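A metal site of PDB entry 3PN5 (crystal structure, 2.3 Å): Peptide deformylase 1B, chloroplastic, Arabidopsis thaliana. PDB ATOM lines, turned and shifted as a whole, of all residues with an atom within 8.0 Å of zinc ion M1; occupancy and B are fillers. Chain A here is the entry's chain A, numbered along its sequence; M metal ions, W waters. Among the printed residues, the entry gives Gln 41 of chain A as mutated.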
ATOM      1  N   ILE A   3       0.268 -11.353   0.035  1.00  0.00           N
ATOM      2  CA  ILE A   3      -0.888 -11.639   0.899  1.00  0.00           C
ATOM      3  C   ILE A   3      -0.564 -12.851   1.779  1.00  0.00           C
ATOM      4  O   ILE A   3      -0.300 -13.941   1.284  1.00  0.00           O
ATOM      5  CB  ILE A   3      -2.132 -11.983   0.042  1.00  0.00           C
ATOM      6  CG1 ILE A   3      -2.658 -10.817  -0.795  1.00  0.00           C
ATOM      7  CG2 ILE A   3      -3.324 -12.449   0.891  1.00  0.00           C
ATOM      8  CD1 ILE A   3      -3.150  -9.629   0.035  1.00  0.00           C
ATOM      9  N   VAL A   4      -0.578 -12.652   3.080  1.00  0.00           N
ATOM     10  CA  VAL A   4      -0.349 -13.753   4.032  1.00  0.00           C
ATOM     11  C   VAL A   4      -1.651 -14.605   4.108  1.00  0.00           C
ATOM     12  O   VAL A   4      -2.772 -14.053   4.165  1.00  0.00           O
ATOM     13  CB  VAL A   4       0.077 -13.135   5.389  1.00  0.00           C
ATOM     14  CG1 VAL A   4       0.058 -14.111   6.563  1.00  0.00           C
ATOM     15  CG2 VAL A   4       1.504 -12.560   5.362  1.00  0.00           C
ATOM     16  N   LEU A  11      -1.638 -13.065  10.769  1.00  0.00           N
ATOM     17  CA  LEU A  11      -3.142 -13.077  10.688  1.00  0.00           C
ATOM     18  C   LEU A  11      -3.844 -13.194  12.079  1.00  0.00           C
ATOM     19  O   LEU A  11      -5.034 -12.862  12.255  1.00  0.00           O
ATOM     20  CB  LEU A  11      -3.660 -14.284   9.889  1.00  0.00           C
ATOM     21  CG  LEU A  11      -3.215 -14.335   8.430  1.00  0.00           C
ATOM     22  CD1 LEU A  11      -3.955 -15.428   7.633  1.00  0.00           C
ATOM     23  CD2 LEU A  11      -3.438 -13.026   7.673  1.00  0.00           C
ATOM     24  N   GLN A  41     -10.333  -6.094  -4.708  1.00  0.00           N
ATOM     25  CA  GLN A  41     -10.911  -6.099  -3.359  1.00  0.00           C
ATOM     26  C   GLN A  41     -11.573  -4.758  -3.033  1.00  0.00           C
ATOM     27  O   GLN A  41     -11.277  -3.723  -3.633  1.00  0.00           O
ATOM     28  CB  GLN A  41      -9.821  -6.363  -2.360  1.00  0.00           C
ATOM     29  CG  GLN A  41      -9.913  -7.745  -1.739  1.00  0.00           C
ATOM     30  CD  GLN A  41      -9.239  -7.788  -0.403  1.00  0.00           C
ATOM     31  OE1 GLN A  41      -8.221  -7.129  -0.222  1.00  0.00           O
ATOM     32  NE2 GLN A  41      -9.752  -8.526   0.557  1.00  0.00           N
ATOM     33  N   GLY A  43     -11.693  -3.795   0.255  1.00  0.00           N
ATOM     34  CA  GLY A  43     -10.961  -3.396   1.472  1.00  0.00           C
ATOM     35  C   GLY A  43      -9.800  -4.362   1.734  1.00  0.00           C
ATOM     36  O   GLY A  43      -9.723  -5.451   1.174  1.00  0.00           O
ATOM     37  N   LEU A  44      -8.869  -3.931   2.601  1.00  0.00           N
ATOM     38  CA  LEU A  44      -7.728  -4.803   2.912  1.00  0.00           C
ATOM     39  C   LEU A  44      -6.913  -4.225   4.081  1.00  0.00           C
ATOM     40  O   LEU A  44      -6.497  -3.066   4.046  1.00  0.00           O
ATOM     41  CB  LEU A  44      -6.827  -4.946   1.677  1.00  0.00           C
ATOM     42  CG  LEU A  44      -5.380  -5.332   2.000  1.00  0.00           C
ATOM     43  CD1 LEU A  44      -5.017  -6.737   1.508  1.00  0.00           C
ATOM     44  CD2 LEU A  44      -4.368  -4.394   1.348  1.00  0.00           C
ATOM     45  N   SER A  45      -6.721  -5.089   5.030  1.00  0.00           N
ATOM     46  CA  SER A  45      -6.009  -4.898   6.308  1.00  0.00           C
ATOM     47  C   SER A  45      -4.500  -5.064   6.167  1.00  0.00           C
ATOM     48  O   SER A  45      -4.003  -5.709   5.249  1.00  0.00           O
ATOM     49  CB  SER A  45      -6.402  -5.961   7.281  1.00  0.00           C
ATOM     50  OG  SER A  45      -5.623  -7.120   7.016  1.00  0.00           O
ATOM     51  N   GLN A  48      -2.918  -8.604   6.543  1.00  0.00           N
ATOM     52  CA  GLN A  48      -3.079  -9.452   5.362  1.00  0.00           C
ATOM     53  C   GLN A  48      -1.919  -9.322   4.437  1.00  0.00           C
ATOM     54  O   GLN A  48      -1.636 -10.214   3.638  1.00  0.00           O
ATOM     55  CB  GLN A  48      -4.332  -9.115   4.625  1.00  0.00           C
ATOM     56  CG  GLN A  48      -5.450  -9.874   5.266  1.00  0.00           C
ATOM     57  CD  GLN A  48      -6.569 -10.238   4.345  1.00  0.00           C
ATOM     58  OE1 GLN A  48      -7.337  -9.357   3.982  1.00  0.00           O
ATOM     59  NE2 GLN A  48      -6.711 -11.482   3.967  1.00  0.00           N
ATOM     60  N   GLU A  89     -19.528 -15.609   2.146  1.00  0.00           N
ATOM     61  CA  GLU A  89     -18.276 -14.837   2.354  1.00  0.00           C
ATOM     62  C   GLU A  89     -17.004 -15.608   1.900  1.00  0.00           C
ATOM     63  O   GLU A  89     -16.964 -16.841   1.907  1.00  0.00           O
ATOM     64  CB  GLU A  89     -18.084 -14.540   3.811  1.00  0.00           C
ATOM     65  CG  GLU A  89     -17.772 -13.092   4.047  1.00  0.00           C
ATOM     66  CD  GLU A  89     -17.504 -12.825   5.498  1.00  0.00           C
ATOM     67  OE1 GLU A  89     -16.349 -13.069   5.987  1.00  0.00           O
ATOM     68  OE2 GLU A  89     -18.448 -12.351   6.233  1.00  0.00           O
ATOM     69  N   GLY A  90     -15.966 -14.798   1.528  1.00  0.00           N
ATOM     70  CA  GLY A  90     -14.648 -15.278   1.044  1.00  0.00           C
ATOM     71  C   GLY A  90     -13.496 -14.448   1.647  1.00  0.00           C
ATOM     72  O   GLY A  90     -13.688 -13.359   2.217  1.00  0.00           O
ATOM     73  N   CYS A  91     -12.275 -14.943   1.506  1.00  0.00           N
ATOM     74  CA  CYS A  91     -11.131 -14.234   2.085  1.00  0.00           C
ATOM     75  C   CYS A  91      -9.843 -14.594   1.344  1.00  0.00           C
ATOM     76  O   CYS A  91      -9.595 -15.782   1.079  1.00  0.00           O
ATOM     77  CB  CYS A  91     -10.965 -14.623   3.551  1.00  0.00           C
ATOM     78  SG  CYS A  91      -9.401 -13.955   4.289  1.00  0.00           S
ATOM     79  N   LEU A  92      -9.059 -13.520   1.071  1.00  0.00           N
ATOM     80  CA  LEU A  92      -7.752 -13.579   0.368  1.00  0.00           C
ATOM     81  C   LEU A  92      -6.732 -14.456   1.126  1.00  0.00           C
ATOM     82  O   LEU A  92      -5.630 -14.714   0.649  1.00  0.00           O
ATOM     83  CB  LEU A  92      -7.143 -12.161   0.233  1.00  0.00           C
ATOM     84  CG  LEU A  92      -6.842 -11.727  -1.216  1.00  0.00           C
ATOM     85  CD1 LEU A  92      -8.075 -11.158  -1.940  1.00  0.00           C
ATOM     86  CD2 LEU A  92      -5.757 -10.639  -1.302  1.00  0.00           C
ATOM     87  N   SER A  93      -7.091 -14.912   2.319  1.00  0.00           N
ATOM     88  CA  SER A  93      -6.188 -15.767   3.113  1.00  0.00           C
ATOM     89  C   SER A  93      -6.525 -17.225   2.934  1.00  0.00           C
ATOM     90  O   SER A  93      -5.665 -18.089   3.183  1.00  0.00           O
ATOM     91  CB  SER A  93      -6.339 -15.471   4.586  1.00  0.00           C
ATOM     92  OG  SER A  93      -5.557 -14.357   4.923  1.00  0.00           O
ATOM     93  N   PHE A  94      -7.699 -17.453   2.577  1.00  0.00           N
ATOM     94  CA  PHE A  94      -8.297 -18.760   2.279  1.00  0.00           C
ATOM     95  C   PHE A  94      -8.720 -18.742   0.799  1.00  0.00           C
ATOM     96  O   PHE A  94      -9.924 -18.676   0.465  1.00  0.00           O
ATOM     97  CB  PHE A  94      -9.510 -18.966   3.228  1.00  0.00           C
ATOM     98  CG  PHE A  94      -9.176 -18.726   4.743  1.00  0.00           C
ATOM     99  CD1 PHE A  94      -9.182 -17.423   5.292  1.00  0.00           C
ATOM    100  CD2 PHE A  94      -8.856 -19.811   5.581  1.00  0.00           C
ATOM    101  CE1 PHE A  94      -8.882 -17.222   6.654  1.00  0.00           C
ATOM    102  CE2 PHE A  94      -8.561 -19.603   6.949  1.00  0.00           C
ATOM    103  CZ  PHE A  94      -8.569 -18.315   7.479  1.00  0.00           C
ATOM    104  N   ARG A 103     -23.461 -11.614   9.724  1.00  0.00           N
ATOM    105  CA  ARG A 103     -22.846 -10.423  10.314  1.00  0.00           C
ATOM    106  C   ARG A 103     -23.877  -9.316  10.321  1.00  0.00           C
ATOM    107  O   ARG A 103     -24.800  -9.289   9.494  1.00  0.00           O
ATOM    108  CB  ARG A 103     -21.603 -10.061   9.520  1.00  0.00           C
ATOM    109  CG  ARG A 103     -20.597 -11.221   9.485  1.00  0.00           C
ATOM    110  CD  ARG A 103     -19.389 -10.953   8.597  1.00  0.00           C
ATOM    111  NE  ARG A 103     -18.347 -10.320   9.364  1.00  0.00           N
ATOM    112  CZ  ARG A 103     -17.102 -10.734   9.490  1.00  0.00           C
ATOM    113  NH1 ARG A 103     -16.642 -11.826   8.865  1.00  0.00           N
ATOM    114  NH2 ARG A 103     -16.228 -10.101  10.258  1.00  0.00           N
ATOM    115  N   ILE A 130     -17.785  -6.103   3.882  1.00  0.00           N
ATOM    116  CA  ILE A 130     -16.364  -6.254   3.607  1.00  0.00           C
ATOM    117  C   ILE A 130     -15.594  -5.531   4.715  1.00  0.00           C
ATOM    118  O   ILE A 130     -14.510  -5.967   5.125  1.00  0.00           O
ATOM    119  CB  ILE A 130     -16.060  -5.705   2.218  1.00  0.00           C
ATOM    120  CG1 ILE A 130     -17.060  -6.200   1.165  1.00  0.00           C
ATOM    121  CG2 ILE A 130     -14.680  -6.120   1.711  1.00  0.00           C
ATOM    122  CD1 ILE A 130     -16.981  -7.717   0.925  1.00  0.00           C
ATOM    123  N   HIS A 133     -15.478  -7.785   7.770  1.00  0.00           N
ATOM    124  CA  HIS A 133     -14.561  -8.862   7.489  1.00  0.00           C
ATOM    125  C   HIS A 133     -13.090  -8.367   7.670  1.00  0.00           C
ATOM    126  O   HIS A 133     -12.241  -9.003   8.248  1.00  0.00           O
ATOM    127  CB  HIS A 133     -14.767  -9.346   6.076  1.00  0.00           C
ATOM    128  CG  HIS A 133     -13.687 -10.307   5.646  1.00  0.00           C
ATOM    129  ND1 HIS A 133     -13.937 -11.660   5.504  1.00  0.00           N
ATOM    130  CD2 HIS A 133     -12.395 -10.109   5.339  1.00  0.00           C
ATOM    131  CE1 HIS A 133     -12.815 -12.236   5.121  1.00  0.00           C
ATOM    132  NE2 HIS A 133     -11.878 -11.318   5.021  1.00  0.00           N
ATOM    133  N   GLU A 134     -12.744  -7.221   7.190  1.00  0.00           N
ATOM    134  CA  GLU A 134     -11.370  -6.718   7.352  1.00  0.00           C
ATOM    135  C   GLU A 134     -11.136  -6.172   8.771  1.00  0.00           C
ATOM    136  O   GLU A 134     -10.000  -5.951   9.206  1.00  0.00           O
ATOM    137  CB  GLU A 134     -11.103  -5.562   6.395  1.00  0.00           C
ATOM    138  CG  GLU A 134     -11.239  -5.960   4.942  1.00  0.00           C
ATOM    139  CD  GLU A 134     -10.261  -7.062   4.553  1.00  0.00           C
ATOM    140  OE1 GLU A 134     -10.658  -8.046   3.822  1.00  0.00           O
ATOM    141  OE2 GLU A 134      -9.039  -6.998   4.959  1.00  0.00           O
ATOM    142  N   TYR A 135     -12.199  -5.971   9.460  1.00  0.00           N
ATOM    143  CA  TYR A 135     -12.080  -5.404  10.799  1.00  0.00           C
ATOM    144  C   TYR A 135     -11.681  -6.504  11.800  1.00  0.00           C
ATOM    145  O   TYR A 135     -11.000  -6.243  12.808  1.00  0.00           O
ATOM    146  CB  TYR A 135     -13.405  -4.797  11.205  1.00  0.00           C
ATOM    147  CG  TYR A 135     -13.338  -4.193  12.579  1.00  0.00           C
ATOM    148  CD1 TYR A 135     -14.226  -4.606  13.560  1.00  0.00           C
ATOM    149  CD2 TYR A 135     -12.368  -3.223  12.852  1.00  0.00           C
ATOM    150  CE1 TYR A 135     -14.166  -4.054  14.835  1.00  0.00           C
ATOM    151  CE2 TYR A 135     -12.299  -2.665  14.127  1.00  0.00           C
ATOM    152  CZ  TYR A 135     -13.200  -3.078  15.114  1.00  0.00           C
ATOM    153  OH  TYR A 135     -13.146  -2.537  16.362  1.00  0.00           O
ATOM    154  N   ASP A 136     -12.163  -7.700  11.488  1.00  0.00           N
ATOM    155  CA  ASP A 136     -11.814  -8.893  12.266  1.00  0.00           C
ATOM    156  C   ASP A 136     -10.369  -9.226  12.057  1.00  0.00           C
ATOM    157  O   ASP A 136      -9.683  -9.752  12.940  1.00  0.00           O
ATOM    158  CB  ASP A 136     -12.654 -10.075  11.824  1.00  0.00           C
ATOM    159  CG  ASP A 136     -14.076 -10.007  12.342  1.00  0.00           C
ATOM    160  OD1 ASP A 136     -14.504  -8.929  12.905  1.00  0.00           O
ATOM    161  OD2 ASP A 136     -14.849 -11.028  12.213  1.00  0.00           O
ATOM    162  N   HIS A 137      -9.939  -8.908  10.853  1.00  0.00           N
ATOM    163  CA  HIS A 137      -8.540  -9.160  10.586  1.00  0.00           C
ATOM    164  C   HIS A 137      -7.710  -8.329  11.607  1.00  0.00           C
ATOM    165  O   HIS A 137      -6.918  -8.873  12.376  1.00  0.00           O
ATOM    166  CB  HIS A 137      -8.268  -8.822   9.101  1.00  0.00           C
ATOM    167  CG  HIS A 137      -8.478 -10.087   8.222  1.00  0.00           C
ATOM    168  ND1 HIS A 137      -7.784 -11.273   8.474  1.00  0.00           N
ATOM    169  CD2 HIS A 137      -9.259 -10.345   7.131  1.00  0.00           C
ATOM    170  CE1 HIS A 137      -8.154 -12.164   7.579  1.00  0.00           C
ATOM    171  NE2 HIS A 137      -9.026 -11.638   6.767  1.00  0.00           N
ATOM    172  N   VAL A 141      -9.086 -12.144  14.171  1.00  0.00           N
ATOM    173  CA  VAL A 141     -10.260 -13.016  13.932  1.00  0.00           C
ATOM    174  C   VAL A 141     -10.384 -13.279  12.408  1.00  0.00           C
ATOM    175  O   VAL A 141     -10.350 -12.345  11.578  1.00  0.00           O
ATOM    176  CB  VAL A 141     -11.568 -12.350  14.473  1.00  0.00           C
ATOM    177  CG1 VAL A 141     -12.788 -13.276  14.391  1.00  0.00           C
ATOM    178  CG2 VAL A 141     -11.483 -11.934  15.950  1.00  0.00           C
ATOM    179  N   LEU A 142     -10.490 -14.578  12.068  1.00  0.00           N
ATOM    180  CA  LEU A 142     -10.633 -15.089  10.683  1.00  0.00           C
ATOM    181  C   LEU A 142     -12.074 -15.633  10.547  1.00  0.00           C
ATOM    182  O   LEU A 142     -12.569 -16.355  11.419  1.00  0.00           O
ATOM    183  CB  LEU A 142      -9.555 -16.139  10.433  1.00  0.00           C
ATOM    184  CG  LEU A 142      -8.146 -15.566  10.614  1.00  0.00           C
ATOM    185  CD1 LEU A 142      -7.045 -16.513  10.118  1.00  0.00           C
ATOM    186  CD2 LEU A 142      -7.916 -14.243   9.864  1.00  0.00           C
ATOM    187  N   PHE A 143     -12.685 -15.373   9.408  1.00  0.00           N
ATOM    188  CA  PHE A 143     -14.139 -15.448   9.166  1.00  0.00           C
ATOM    189  C   PHE A 143     -14.736 -16.840   9.534  1.00  0.00           C
ATOM    190  O   PHE A 143     -15.931 -16.952   9.824  1.00  0.00           O
ATOM    191  CB  PHE A 143     -14.476 -15.137   7.685  1.00  0.00           C
ATOM    192  CG  PHE A 143     -13.971 -16.131   6.602  1.00  0.00           C
ATOM    193  CD1 PHE A 143     -12.817 -16.904   6.797  1.00  0.00           C
ATOM    194  CD2 PHE A 143     -14.698 -16.247   5.398  1.00  0.00           C
ATOM    195  CE1 PHE A 143     -12.390 -17.794   5.773  1.00  0.00           C
ATOM    196  CE2 PHE A 143     -14.268 -17.121   4.393  1.00  0.00           C
ATOM    197  CZ  PHE A 143     -13.114 -17.896   4.574  1.00  0.00           C
HETATM  198 ZN    ZN M   1     -10.118 -12.018   4.875  1.00  0.00          ZN
HETATM  199 ZN    ZN M   2      -9.178  -9.133   3.141  1.00  0.00          ZN
HETATM  200  O   HOH W   1      -9.583 -10.715   3.918  1.00  0.00           O
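Zinc ion M1 is bound by water W1 (1.7 Å), a ring nitrogen (NE2) of His 133 (1.9 Å), the side-chain sulfur (SG) of Cys 91 (2.1 Å) and a ring nitrogen (NE2) of His 137 (2.2 Å). Zinc ion M1 has four donor atoms within binding distance.
Gln 48 touches zinc ion M1. Four residues have an atom within 4 Å of zinc ion M1: Gln 48, Cys 91, His 133 and His 137. Along chain A the residues within 4 Å of zinc ion M1 span positions 48 to 137. The nearest printed residue that does not touch zinc ion M1 is Glu 134 (4.1 Å).
OE1 of Glu 89 is in hydrogen-bond range of ND1 of His 133 (2.8 Å). The side-chain sulfur of Cys 91 lies close to the side-chain amide nitrogen of Gln 48, 3.7 Å away. The side-chain sulfur (SG) of Cys 91 sits close to the backbone NH (N) of Ser 93 (3.2 Å). OG of Ser 93 is in hydrogen-bond range of NE2 of Gln 48. OG of Ser 45 lies within hydrogen-bond range of N of Gln 48 (3.1 Å). The backbone NH (N) of Val 4 sits at hydrogen-bond distance from the backbone carbonyl oxygen (O) of Gln 48 (2.7 Å).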
